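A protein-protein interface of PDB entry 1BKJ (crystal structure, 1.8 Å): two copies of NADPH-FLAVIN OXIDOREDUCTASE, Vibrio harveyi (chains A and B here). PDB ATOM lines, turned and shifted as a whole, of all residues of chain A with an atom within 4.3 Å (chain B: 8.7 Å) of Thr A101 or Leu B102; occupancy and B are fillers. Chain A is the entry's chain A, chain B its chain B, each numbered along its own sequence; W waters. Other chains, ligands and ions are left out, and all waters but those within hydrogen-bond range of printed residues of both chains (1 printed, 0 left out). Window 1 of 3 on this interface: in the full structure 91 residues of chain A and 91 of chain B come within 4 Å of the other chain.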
ATOM      1  N   ILE A  81      -7.404  -4.999 -25.509  1.00  0.00           N
ATOM      2  CA  ILE A  81      -8.133  -5.969 -24.667  1.00  0.00           C
ATOM      3  C   ILE A  81      -9.579  -5.459 -24.767  1.00  0.00           C
ATOM      4  O   ILE A  81      -9.809  -4.244 -24.711  1.00  0.00           O
ATOM      5  CB  ILE A  81      -7.717  -5.914 -23.154  1.00  0.00           C
ATOM      6  CG1 ILE A  81      -6.256  -6.322 -22.975  1.00  0.00           C
ATOM      7  CG2 ILE A  81      -8.639  -6.824 -22.321  1.00  0.00           C
ATOM      8  CD1 ILE A  81      -5.709  -6.133 -21.583  1.00  0.00           C
ATOM      9  N   PHE A  97     -11.028  -8.836 -12.791  1.00  0.00           N
ATOM     10  CA  PHE A  97     -10.043  -9.772 -12.257  1.00  0.00           C
ATOM     11  C   PHE A  97      -8.781  -9.757 -13.131  1.00  0.00           C
ATOM     12  O   PHE A  97      -8.879  -9.803 -14.365  1.00  0.00           O
ATOM     13  CB  PHE A  97     -10.627 -11.182 -12.199  1.00  0.00           C
ATOM     14  CG  PHE A  97     -11.680 -11.352 -11.157  1.00  0.00           C
ATOM     15  CD1 PHE A  97     -11.326 -11.638  -9.823  1.00  0.00           C
ATOM     16  CD2 PHE A  97     -13.040 -11.231 -11.497  1.00  0.00           C
ATOM     17  CE1 PHE A  97     -12.315 -11.807  -8.829  1.00  0.00           C
ATOM     18  CE2 PHE A  97     -14.046 -11.396 -10.520  1.00  0.00           C
ATOM     19  CZ  PHE A  97     -13.682 -11.686  -9.173  1.00  0.00           C
ATOM     20  N   THR A  98      -7.606  -9.693 -12.493  1.00  0.00           N
ATOM     21  CA  THR A  98      -6.295  -9.672 -13.177  1.00  0.00           C
ATOM     22  C   THR A  98      -6.131 -10.827 -14.179  1.00  0.00           C
ATOM     23  O   THR A  98      -5.490 -10.650 -15.216  1.00  0.00           O
ATOM     24  CB  THR A  98      -5.139  -9.611 -12.139  1.00  0.00           C
ATOM     25  OG1 THR A  98      -5.278  -8.406 -11.372  1.00  0.00           O
ATOM     26  CG2 THR A  98      -3.757  -9.609 -12.800  1.00  0.00           C
ATOM     27  N   GLU A  99      -6.781 -11.965 -13.901  1.00  0.00           N
ATOM     28  CA  GLU A  99      -6.776 -13.144 -14.781  1.00  0.00           C
ATOM     29  C   GLU A  99      -7.226 -12.772 -16.198  1.00  0.00           C
ATOM     30  O   GLU A  99      -6.635 -13.203 -17.186  1.00  0.00           O
ATOM     31  CB  GLU A  99      -7.717 -14.215 -14.202  1.00  0.00           C
ATOM     32  CG  GLU A  99      -8.193 -15.339 -15.149  1.00  0.00           C
ATOM     33  CD  GLU A  99      -7.108 -16.305 -15.593  1.00  0.00           C
ATOM     34  OE1 GLU A  99      -5.962 -16.236 -15.099  1.00  0.00           O
ATOM     35  OE2 GLU A  99      -7.417 -17.168 -16.439  1.00  0.00           O
ATOM     36  N   LEU A 100      -8.251 -11.929 -16.261  1.00  0.00           N
ATOM     37  CA  LEU A 100      -8.826 -11.472 -17.517  1.00  0.00           C
ATOM     38  C   LEU A 100      -7.908 -10.544 -18.325  1.00  0.00           C
ATOM     39  O   LEU A 100      -7.898 -10.593 -19.558  1.00  0.00           O
ATOM     40  CB  LEU A 100     -10.217 -10.884 -17.258  1.00  0.00           C
ATOM     41  CG  LEU A 100     -11.193 -11.914 -16.665  1.00  0.00           C
ATOM     42  CD1 LEU A 100     -12.530 -11.282 -16.458  1.00  0.00           C
ATOM     43  CD2 LEU A 100     -11.322 -13.164 -17.534  1.00  0.00           C
ATOM     44  N   THR A 101      -7.088  -9.769 -17.615  1.00  0.00           N
ATOM     45  CA  THR A 101      -6.104  -8.881 -18.235  1.00  0.00           C
ATOM     46  C   THR A 101      -4.939  -9.754 -18.748  1.00  0.00           C
ATOM     47  O   THR A 101      -4.399  -9.481 -19.824  1.00  0.00           O
ATOM     48  CB  THR A 101      -5.650  -7.753 -17.247  1.00  0.00           C
ATOM     49  OG1 THR A 101      -6.742  -6.840 -17.060  1.00  0.00           O
ATOM     50  CG2 THR A 101      -4.437  -6.971 -17.768  1.00  0.00           C
ATOM     51  N   LEU A 102      -4.605 -10.830 -18.015  1.00  0.00           N
ATOM     52  CA  LEU A 102      -3.549 -11.753 -18.433  1.00  0.00           C
ATOM     53  C   LEU A 102      -3.969 -12.462 -19.702  1.00  0.00           C
ATOM     54  O   LEU A 102      -3.154 -12.613 -20.609  1.00  0.00           O
ATOM     55  CB  LEU A 102      -3.239 -12.824 -17.388  1.00  0.00           C
ATOM     56  CG  LEU A 102      -2.416 -12.539 -16.139  1.00  0.00           C
ATOM     57  CD1 LEU A 102      -1.960 -13.890 -15.580  1.00  0.00           C
ATOM     58  CD2 LEU A 102      -1.197 -11.657 -16.466  1.00  0.00           C
ATOM     59  N   ILE A 103      -5.247 -12.858 -19.771  1.00  0.00           N
ATOM     60  CA  ILE A 103      -5.810 -13.532 -20.955  1.00  0.00           C
ATOM     61  C   ILE A 103      -5.786 -12.551 -22.123  1.00  0.00           C
ATOM     62  O   ILE A 103      -5.369 -12.924 -23.212  1.00  0.00           O
ATOM     63  CB  ILE A 103      -7.257 -14.078 -20.701  1.00  0.00           C
ATOM     64  CG1 ILE A 103      -7.170 -15.393 -19.933  1.00  0.00           C
ATOM     65  CG2 ILE A 103      -8.041 -14.315 -22.030  1.00  0.00           C
ATOM     66  CD1 ILE A 103      -8.531 -15.922 -19.471  1.00  0.00           C
ATOM     67  N   GLY A 104      -6.184 -11.302 -21.865  1.00  0.00           N
ATOM     68  CA  GLY A 104      -6.177 -10.265 -22.886  1.00  0.00           C
ATOM     69  C   GLY A 104      -4.798 -10.023 -23.490  1.00  0.00           C
ATOM     70  O   GLY A 104      -4.675  -9.941 -24.707  1.00  0.00           O
ATOM     71  N   ALA A 105      -3.768  -9.975 -22.645  1.00  0.00           N
ATOM     72  CA  ALA A 105      -2.384  -9.769 -23.081  1.00  0.00           C
ATOM     73  C   ALA A 105      -1.790 -10.966 -23.840  1.00  0.00           C
ATOM     74  O   ALA A 105      -1.165 -10.785 -24.889  1.00  0.00           O
ATOM     75  CB  ALA A 105      -1.514  -9.400 -21.895  1.00  0.00           C
ATOM     76  N   ILE A 228       0.790   2.691 -15.584  1.00  0.00           N
ATOM     77  CA  ILE A 228       0.089   1.556 -16.188  1.00  0.00           C
ATOM     78  C   ILE A 228      -1.016   0.892 -15.356  1.00  0.00           C
ATOM     79  O   ILE A 228      -2.105   0.664 -15.905  1.00  0.00           O
ATOM     80  CB  ILE A 228       1.117   0.541 -16.843  1.00  0.00           C
ATOM     81  CG1 ILE A 228       1.688   1.153 -18.130  1.00  0.00           C
ATOM     82  CG2 ILE A 228       0.505  -0.863 -17.117  1.00  0.00           C
ATOM     83  CD1 ILE A 228       0.672   1.410 -19.244  1.00  0.00           C
ATOM     84  N   LEU A 232      -5.035   0.924 -16.245  1.00  0.00           N
ATOM     85  CA  LEU A 232      -5.856  -0.280 -16.365  1.00  0.00           C
ATOM     86  C   LEU A 232      -7.058  -0.193 -15.423  1.00  0.00           C
ATOM     87  O   LEU A 232      -8.184  -0.411 -15.861  1.00  0.00           O
ATOM     88  CB  LEU A 232      -5.028  -1.542 -16.088  1.00  0.00           C
ATOM     89  CG  LEU A 232      -3.987  -1.985 -17.138  1.00  0.00           C
ATOM     90  CD1 LEU A 232      -3.199  -3.179 -16.626  1.00  0.00           C
ATOM     91  CD2 LEU A 232      -4.646  -2.322 -18.483  1.00  0.00           C
ATOM     92  N   LEU A 237     -10.145  -2.502 -15.346  1.00  0.00           N
ATOM     93  CA  LEU A 237      -9.400  -3.753 -15.465  1.00  0.00           C
ATOM     94  C   LEU A 237      -8.383  -3.944 -14.343  1.00  0.00           C
ATOM     95  O   LEU A 237      -7.953  -2.971 -13.725  1.00  0.00           O
ATOM     96  CB  LEU A 237      -8.690  -3.794 -16.824  1.00  0.00           C
ATOM     97  CG  LEU A 237      -9.580  -3.725 -18.073  1.00  0.00           C
ATOM     98  CD1 LEU A 237      -8.744  -3.525 -19.303  1.00  0.00           C
ATOM     99  CD2 LEU A 237     -10.416  -4.997 -18.189  1.00  0.00           C
ATOM    100  N   ALA A 238      -8.042  -5.203 -14.062  1.00  0.00           N
ATOM    101  CA  ALA A 238      -7.043  -5.595 -13.053  1.00  0.00           C
ATOM    102  C   ALA A 238      -7.111  -4.892 -11.688  1.00  0.00           C
ATOM    103  O   ALA A 238      -6.110  -4.352 -11.188  1.00  0.00           O
ATOM    104  CB  ALA A 238      -5.623  -5.490 -13.658  1.00  0.00           C
ATOM    105  N   SER B  40      10.008  -7.333 -26.695  1.00  0.00           N
ATOM    106  CA  SER B  40       9.845  -5.958 -26.193  1.00  0.00           C
ATOM    107  C   SER B  40      11.149  -5.445 -25.611  1.00  0.00           C
ATOM    108  O   SER B  40      11.669  -6.041 -24.660  1.00  0.00           O
ATOM    109  CB  SER B  40       8.777  -5.894 -25.101  1.00  0.00           C
ATOM    110  OG  SER B  40       7.530  -6.401 -25.539  1.00  0.00           O
ATOM    111  N   VAL B  45      12.227 -11.873 -21.885  1.00  0.00           N
ATOM    112  CA  VAL B  45      11.661 -12.225 -20.581  1.00  0.00           C
ATOM    113  C   VAL B  45      10.858 -13.525 -20.506  1.00  0.00           C
ATOM    114  O   VAL B  45      10.076 -13.741 -19.573  1.00  0.00           O
ATOM    115  CB  VAL B  45      10.807 -11.035 -20.044  1.00  0.00           C
ATOM    116  CG1 VAL B  45      11.644  -9.797 -20.015  1.00  0.00           C
ATOM    117  CG2 VAL B  45       9.565 -10.796 -20.913  1.00  0.00           C
ATOM    118  N   ILE B  81       7.010 -16.144 -17.325  1.00  0.00           N
ATOM    119  CA  ILE B  81       7.537 -14.779 -17.295  1.00  0.00           C
ATOM    120  C   ILE B  81       8.841 -14.974 -16.505  1.00  0.00           C
ATOM    121  O   ILE B  81       8.844 -15.711 -15.515  1.00  0.00           O
ATOM    122  CB  ILE B  81       6.624 -13.834 -16.475  1.00  0.00           C
ATOM    123  CG1 ILE B  81       5.287 -13.658 -17.183  1.00  0.00           C
ATOM    124  CG2 ILE B  81       7.292 -12.464 -16.251  1.00  0.00           C
ATOM    125  CD1 ILE B  81       4.278 -12.817 -16.436  1.00  0.00           C
ATOM    126  N   TYR B  83      12.071 -12.619 -14.996  1.00  0.00           N
ATOM    127  CA  TYR B  83      12.874 -11.422 -14.733  1.00  0.00           C
ATOM    128  C   TYR B  83      13.994 -11.786 -13.740  1.00  0.00           C
ATOM    129  O   TYR B  83      14.695 -10.908 -13.217  1.00  0.00           O
ATOM    130  CB  TYR B  83      12.013 -10.283 -14.182  1.00  0.00           C
ATOM    131  CG  TYR B  83      11.204  -9.581 -15.238  1.00  0.00           C
ATOM    132  CD1 TYR B  83      11.796  -8.583 -16.050  1.00  0.00           C
ATOM    133  CD2 TYR B  83       9.858  -9.939 -15.483  1.00  0.00           C
ATOM    134  CE1 TYR B  83      11.069  -7.958 -17.086  1.00  0.00           C
ATOM    135  CE2 TYR B  83       9.115  -9.314 -16.529  1.00  0.00           C
ATOM    136  CZ  TYR B  83       9.737  -8.331 -17.328  1.00  0.00           C
ATOM    137  OH  TYR B  83       9.059  -7.745 -18.376  1.00  0.00           O
ATOM    138  N   ALA B  95      11.445  -5.443 -10.679  1.00  0.00           N
ATOM    139  CA  ALA B  95      10.587  -6.262 -11.545  1.00  0.00           C
ATOM    140  C   ALA B  95       9.101  -6.288 -11.199  1.00  0.00           C
ATOM    141  O   ALA B  95       8.317  -6.946 -11.884  1.00  0.00           O
ATOM    142  CB  ALA B  95      11.121  -7.677 -11.591  1.00  0.00           C
ATOM    143  N   PHE B  97       6.692  -3.782 -11.316  1.00  0.00           N
ATOM    144  CA  PHE B  97       5.748  -2.912 -12.035  1.00  0.00           C
ATOM    145  C   PHE B  97       4.841  -3.730 -12.968  1.00  0.00           C
ATOM    146  O   PHE B  97       5.331  -4.617 -13.681  1.00  0.00           O
ATOM    147  CB  PHE B  97       6.520  -1.854 -12.837  1.00  0.00           C
ATOM    148  CG  PHE B  97       7.139  -0.772 -11.985  1.00  0.00           C
ATOM    149  CD1 PHE B  97       6.360   0.315 -11.525  1.00  0.00           C
ATOM    150  CD2 PHE B  97       8.504  -0.833 -11.629  1.00  0.00           C
ATOM    151  CE1 PHE B  97       6.930   1.334 -10.716  1.00  0.00           C
ATOM    152  CE2 PHE B  97       9.096   0.181 -10.818  1.00  0.00           C
ATOM    153  CZ  PHE B  97       8.304   1.265 -10.363  1.00  0.00           C
ATOM    154  N   THR B  98       3.535  -3.436 -12.954  1.00  0.00           N
ATOM    155  CA  THR B  98       2.531  -4.142 -13.779  1.00  0.00           C
ATOM    156  C   THR B  98       2.881  -4.179 -15.273  1.00  0.00           C
ATOM    157  O   THR B  98       2.650  -5.188 -15.951  1.00  0.00           O
ATOM    158  CB  THR B  98       1.113  -3.570 -13.530  1.00  0.00           C
ATOM    159  OG1 THR B  98       0.780  -3.778 -12.152  1.00  0.00           O
ATOM    160  CG2 THR B  98       0.036  -4.272 -14.391  1.00  0.00           C
ATOM    161  N   GLU B  99       3.531  -3.110 -15.740  1.00  0.00           N
ATOM    162  CA  GLU B  99       4.000  -2.984 -17.124  1.00  0.00           C
ATOM    163  C   GLU B  99       4.864  -4.184 -17.502  1.00  0.00           C
ATOM    164  O   GLU B  99       4.700  -4.752 -18.584  1.00  0.00           O
ATOM    165  CB  GLU B  99       4.799  -1.673 -17.296  1.00  0.00           C
ATOM    166  CG  GLU B  99       5.742  -1.583 -18.517  1.00  0.00           C
ATOM    167  CD  GLU B  99       5.021  -1.419 -19.849  1.00  0.00           C
ATOM    168  OE1 GLU B  99       3.776  -1.363 -19.898  1.00  0.00           O
ATOM    169  OE2 GLU B  99       5.717  -1.306 -20.870  1.00  0.00           O
ATOM    170  N   LEU B 100       5.712  -4.611 -16.567  1.00  0.00           N
ATOM    171  CA  LEU B 100       6.604  -5.743 -16.783  1.00  0.00           C
ATOM    172  C   LEU B 100       5.887  -7.093 -16.874  1.00  0.00           C
ATOM    173  O   LEU B 100       6.365  -7.994 -17.564  1.00  0.00           O
ATOM    174  CB  LEU B 100       7.754  -5.738 -15.754  1.00  0.00           C
ATOM    175  CG  LEU B 100       8.595  -4.450 -15.781  1.00  0.00           C
ATOM    176  CD1 LEU B 100       9.666  -4.488 -14.736  1.00  0.00           C
ATOM    177  CD2 LEU B 100       9.235  -4.208 -17.141  1.00  0.00           C
ATOM    178  N   THR B 101       4.727  -7.215 -16.224  1.00  0.00           N
ATOM    179  CA  THR B 101       3.919  -8.439 -16.292  1.00  0.00           C
ATOM    180  C   THR B 101       3.158  -8.447 -17.633  1.00  0.00           C
ATOM    181  O   THR B 101       2.978  -9.507 -18.237  1.00  0.00           O
ATOM    182  CB  THR B 101       2.933  -8.552 -15.094  1.00  0.00           C
ATOM    183  OG1 THR B 101       3.685  -8.654 -13.884  1.00  0.00           O
ATOM    184  CG2 THR B 101       2.045  -9.816 -15.199  1.00  0.00           C
ATOM    185  N   LEU B 102       2.759  -7.264 -18.111  1.00  0.00           N
ATOM    186  CA  LEU B 102       2.077  -7.143 -19.405  1.00  0.00           C
ATOM    187  C   LEU B 102       3.031  -7.509 -20.533  1.00  0.00           C
ATOM    188  O   LEU B 102       2.623  -8.197 -21.454  1.00  0.00           O
ATOM    189  CB  LEU B 102       1.544  -5.729 -19.649  1.00  0.00           C
ATOM    190  CG  LEU B 102       0.342  -5.213 -18.857  1.00  0.00           C
ATOM    191  CD1 LEU B 102       0.034  -3.808 -19.368  1.00  0.00           C
ATOM    192  CD2 LEU B 102      -0.873  -6.137 -19.003  1.00  0.00           C
ATOM    193  N   ILE B 103       4.301  -7.092 -20.423  1.00  0.00           N
ATOM    194  CA  ILE B 103       5.360  -7.407 -21.414  1.00  0.00           C
ATOM    195  C   ILE B 103       5.598  -8.917 -21.407  1.00  0.00           C
ATOM    196  O   ILE B 103       5.694  -9.533 -22.461  1.00  0.00           O
ATOM    197  CB  ILE B 103       6.703  -6.666 -21.093  1.00  0.00           C
ATOM    198  CG1 ILE B 103       6.593  -5.195 -21.481  1.00  0.00           C
ATOM    199  CG2 ILE B 103       7.908  -7.322 -21.795  1.00  0.00           C
ATOM    200  CD1 ILE B 103       7.769  -4.345 -21.031  1.00  0.00           C
ATOM    201  N   GLY B 104       5.653  -9.492 -20.203  1.00  0.00           N
ATOM    202  CA  GLY B 104       5.853 -10.925 -20.035  1.00  0.00           C
ATOM    203  C   GLY B 104       4.749 -11.755 -20.671  1.00  0.00           C
ATOM    204  O   GLY B 104       5.035 -12.725 -21.374  1.00  0.00           O
ATOM    205  N   ALA B 105       3.498 -11.338 -20.462  1.00  0.00           N
ATOM    206  CA  ALA B 105       2.333 -12.020 -21.024  1.00  0.00           C
ATOM    207  C   ALA B 105       2.237 -11.884 -22.560  1.00  0.00           C
ATOM    208  O   ALA B 105       2.037 -12.885 -23.260  1.00  0.00           O
ATOM    209  CB  ALA B 105       1.071 -11.518 -20.351  1.00  0.00           C
ATOM    210  N   VAL B 106       2.435 -10.666 -23.077  1.00  0.00           N
ATOM    211  CA  VAL B 106       2.385 -10.406 -24.522  1.00  0.00           C
ATOM    212  C   VAL B 106       3.507 -11.165 -25.235  1.00  0.00           C
ATOM    213  O   VAL B 106       3.225 -11.903 -26.169  1.00  0.00           O
ATOM    214  CB  VAL B 106       2.471  -8.867 -24.864  1.00  0.00           C
ATOM    215  CG1 VAL B 106       2.704  -8.638 -26.365  1.00  0.00           C
ATOM    216  CG2 VAL B 106       1.185  -8.157 -24.451  1.00  0.00           C
ATOM    217  N   ASP B 107       4.749 -11.007 -24.759  1.00  0.00           N
ATOM    218  CA  ASP B 107       5.918 -11.674 -25.347  1.00  0.00           C
ATOM    219  C   ASP B 107       5.844 -13.205 -25.331  1.00  0.00           C
ATOM    220  O   ASP B 107       6.326 -13.843 -26.267  1.00  0.00           O
ATOM    221  CB  ASP B 107       7.219 -11.177 -24.707  1.00  0.00           C
ATOM    222  CG  ASP B 107       7.587  -9.740 -25.116  1.00  0.00           C
ATOM    223  OD1 ASP B 107       6.743  -8.975 -25.634  1.00  0.00           O
ATOM    224  OD2 ASP B 107       8.756  -9.363 -24.912  1.00  0.00           O
ATOM    225  N   SER B 108       5.200 -13.781 -24.305  1.00  0.00           N
ATOM    226  CA  SER B 108       5.013 -15.236 -24.190  1.00  0.00           C
ATOM    227  C   SER B 108       4.032 -15.737 -25.243  1.00  0.00           C
ATOM    228  O   SER B 108       4.215 -16.825 -25.794  1.00  0.00           O
ATOM    229  CB  SER B 108       4.452 -15.625 -22.825  1.00  0.00           C
ATOM    230  OG  SER B 108       5.369 -15.349 -21.794  1.00  0.00           O
ATOM    231  N   GLY B 109       2.983 -14.942 -25.482  1.00  0.00           N
ATOM    232  CA  GLY B 109       1.962 -15.260 -26.470  1.00  0.00           C
ATOM    233  C   GLY B 109       2.543 -15.271 -27.874  1.00  0.00           C
ATOM    234  O   GLY B 109       2.286 -16.193 -28.644  1.00  0.00           O
ATOM    235  N   ILE B 110       3.396 -14.287 -28.162  1.00  0.00           N
ATOM    236  CA  ILE B 110       4.085 -14.145 -29.449  1.00  0.00           C
ATOM    237  C   ILE B 110       5.040 -15.326 -29.669  1.00  0.00           C
ATOM    238  O   ILE B 110       5.005 -15.955 -30.732  1.00  0.00           O
ATOM    239  CB  ILE B 110       4.895 -12.817 -29.516  1.00  0.00           C
ATOM    240  CG1 ILE B 110       3.948 -11.620 -29.415  1.00  0.00           C
ATOM    241  CG2 ILE B 110       5.665 -12.714 -30.833  1.00  0.00           C
ATOM    242  CD1 ILE B 110       4.624 -10.285 -29.200  1.00  0.00           C
ATOM    243  N   ARG B 133      -3.103 -22.477 -14.589  1.00  0.00           N
ATOM    244  CA  ARG B 133      -3.370 -21.364 -13.692  1.00  0.00           C
ATOM    245  C   ARG B 133      -4.391 -21.684 -12.594  1.00  0.00           C
ATOM    246  O   ARG B 133      -4.481 -20.948 -11.618  1.00  0.00           O
ATOM    247  CB  ARG B 133      -3.742 -20.099 -14.470  1.00  0.00           C
ATOM    248  CG  ARG B 133      -2.611 -19.589 -15.349  1.00  0.00           C
ATOM    249  CD  ARG B 133      -2.741 -18.106 -15.723  1.00  0.00           C
ATOM    250  NE  ARG B 133      -3.975 -17.767 -16.441  1.00  0.00           N
ATOM    251  CZ  ARG B 133      -4.238 -18.029 -17.725  1.00  0.00           C
ATOM    252  NH1 ARG B 133      -3.361 -18.650 -18.505  1.00  0.00           N
ATOM    253  NH2 ARG B 133      -5.405 -17.663 -18.234  1.00  0.00           N
ATOM    254  N   LEU B 152       2.518 -19.007 -16.836  1.00  0.00           N
ATOM    255  CA  LEU B 152       1.400 -18.430 -17.565  1.00  0.00           C
ATOM    256  C   LEU B 152       0.502 -19.484 -18.189  1.00  0.00           C
ATOM    257  O   LEU B 152      -0.709 -19.476 -17.977  1.00  0.00           O
ATOM    258  CB  LEU B 152       1.895 -17.478 -18.635  1.00  0.00           C
ATOM    259  CG  LEU B 152       2.506 -16.175 -18.164  1.00  0.00           C
ATOM    260  CD1 LEU B 152       2.919 -15.440 -19.394  1.00  0.00           C
ATOM    261  CD2 LEU B 152       1.535 -15.342 -17.331  1.00  0.00           C
ATOM    262  N   SER B 224     -13.320 -15.096 -12.047  1.00  0.00           N
ATOM    263  CA  SER B 224     -12.304 -15.685 -12.915  1.00  0.00           C
ATOM    264  C   SER B 224     -10.973 -15.774 -12.198  1.00  0.00           C
ATOM    265  O   SER B 224     -10.299 -14.755 -12.022  1.00  0.00           O
ATOM    266  CB  SER B 224     -12.149 -14.861 -14.190  1.00  0.00           C
ATOM    267  OG  SER B 224     -13.327 -14.890 -14.974  1.00  0.00           O
ATOM    268  N   ILE B 228      -5.157 -15.365  -8.819  1.00  0.00           N
ATOM    269  CA  ILE B 228      -4.086 -14.946  -9.730  1.00  0.00           C
ATOM    270  C   ILE B 228      -3.225 -13.732  -9.362  1.00  0.00           C
ATOM    271  O   ILE B 228      -1.999 -13.849  -9.443  1.00  0.00           O
ATOM    272  CB  ILE B 228      -4.572 -14.979 -11.219  1.00  0.00           C
ATOM    273  CG1 ILE B 228      -4.700 -16.442 -11.667  1.00  0.00           C
ATOM    274  CG2 ILE B 228      -3.657 -14.181 -12.170  1.00  0.00           C
ATOM    275  CD1 ILE B 228      -3.403 -17.267 -11.642  1.00  0.00           C
ATOM    276  N   LEU B 232       0.886 -13.819  -8.501  1.00  0.00           N
ATOM    277  CA  LEU B 232       1.895 -12.971  -9.143  1.00  0.00           C
ATOM    278  C   LEU B 232       2.625 -12.143  -8.084  1.00  0.00           C
ATOM    279  O   LEU B 232       3.856 -12.076  -8.104  1.00  0.00           O
ATOM    280  CB  LEU B 232       1.243 -12.035 -10.178  1.00  0.00           C
ATOM    281  CG  LEU B 232       0.592 -12.661 -11.421  1.00  0.00           C
ATOM    282  CD1 LEU B 232      -0.151 -11.584 -12.217  1.00  0.00           C
ATOM    283  CD2 LEU B 232       1.652 -13.356 -12.266  1.00  0.00           C
ATOM    284  N   LEU B 237       5.811 -10.008  -8.628  1.00  0.00           N
ATOM    285  CA  LEU B 237       5.326  -9.386  -9.860  1.00  0.00           C
ATOM    286  C   LEU B 237       3.978  -8.686  -9.691  1.00  0.00           C
ATOM    287  O   LEU B 237       3.201  -9.052  -8.820  1.00  0.00           O
ATOM    288  CB  LEU B 237       5.236 -10.446 -10.973  1.00  0.00           C
ATOM    289  CG  LEU B 237       6.534 -11.170 -11.377  1.00  0.00           C
ATOM    290  CD1 LEU B 237       6.223 -12.372 -12.237  1.00  0.00           C
ATOM    291  CD2 LEU B 237       7.506 -10.227 -12.079  1.00  0.00           C
ATOM    292  N   ALA B 238       3.732  -7.657 -10.507  1.00  0.00           N
ATOM    293  CA  ALA B 238       2.481  -6.895 -10.521  1.00  0.00           C
ATOM    294  C   ALA B 238       2.026  -6.329  -9.176  1.00  0.00           C
ATOM    295  O   ALA B 238       0.837  -6.378  -8.838  1.00  0.00           O
ATOM    296  CB  ALA B 238       1.365  -7.725 -11.171  1.00  0.00           C
HETATM  297  O   HOH W   1      -7.796 -12.820 -11.240  1.00  0.00           O
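O of Ser B224 touches CB of Phe A97 (3.6 Å). Ile B228 touches Glu A99 (CG1 to OE1, 3.7 Å). Leu A100 touches Ser B224 (CD2 to OG, 3.7 Å). Thr A101 touches Leu B102 (CG2 to CD2, 3.9 Å). CD2 of Leu A102 touches CG2 of Thr B101, 3.9 Å away. Leu A102 touches Ile B228 (CD1 to CG2, 3.8 Å). Arg B133 touches Ile A103 (NH2 to CG1, 3.3 Å). CB of Ala A105 touches CB of Ala B105, at 3.7 Å. CG1 of Ile A228 touches OE1 of Glu B99 (3.7 Å). CD1 of Leu B102 touches CG2 of Ile A228 (3.7 Å).
O of Leu B152 lies within hydrogen-bond range of NH1 of Arg B133 (2.8 Å).
Water W1 lies within hydrogen-bond range of the backbone NH (N) of Glu A99 (3.0 Å), the backbone carbonyl oxygen (O) of Ser B224 (3.3 Å) and the backbone NH (N) of Thr A98 (3.4 Å).
Of chain B, only Leu B102 comes within 4 Å of Thr A101. Of the printed residues of chain A, Leu B102 touches Thr A101 and Ile A228. Printed residues of chain B within 4 Å of Ile A103: Arg B133 (3.3 Å). Printed residues of chain B within 4 Å of Leu A100: Ser B224. Gly B104 touches none of the printed residues of chain A. The nearest residue of chain B that does not touch Thr A101 is Ala B105 (5.9 Å).
Glu A99 touches Ile B228, and with the chains exchanged Ile A228 touches Glu B99. Thr A101 touches Leu B102, and with the chains exchanged Leu A102 touches Thr B101. Leu A102 touches Ile B228, and with the chains exchanged Ile A228 touches Leu B102. Ala A105 touches its own counterpart, Ala B105.
The guanidinium group of Arg B133 is in salt-bridge range of the side-chain carboxylate of Glu A99 (2.7 Å).
Hydrophobic or aromatic side chains of chain B that line the printed part of chain A: Leu B102, Ala B105, Val B106 and Ile B228. Among the printed residues, 13 pairs touch across the chains. Among the printed residues, Asp or Glu carboxylates within 4 Å of a Lys or Arg side-chain nitrogen of the other chain: Glu A99 with Arg B133.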
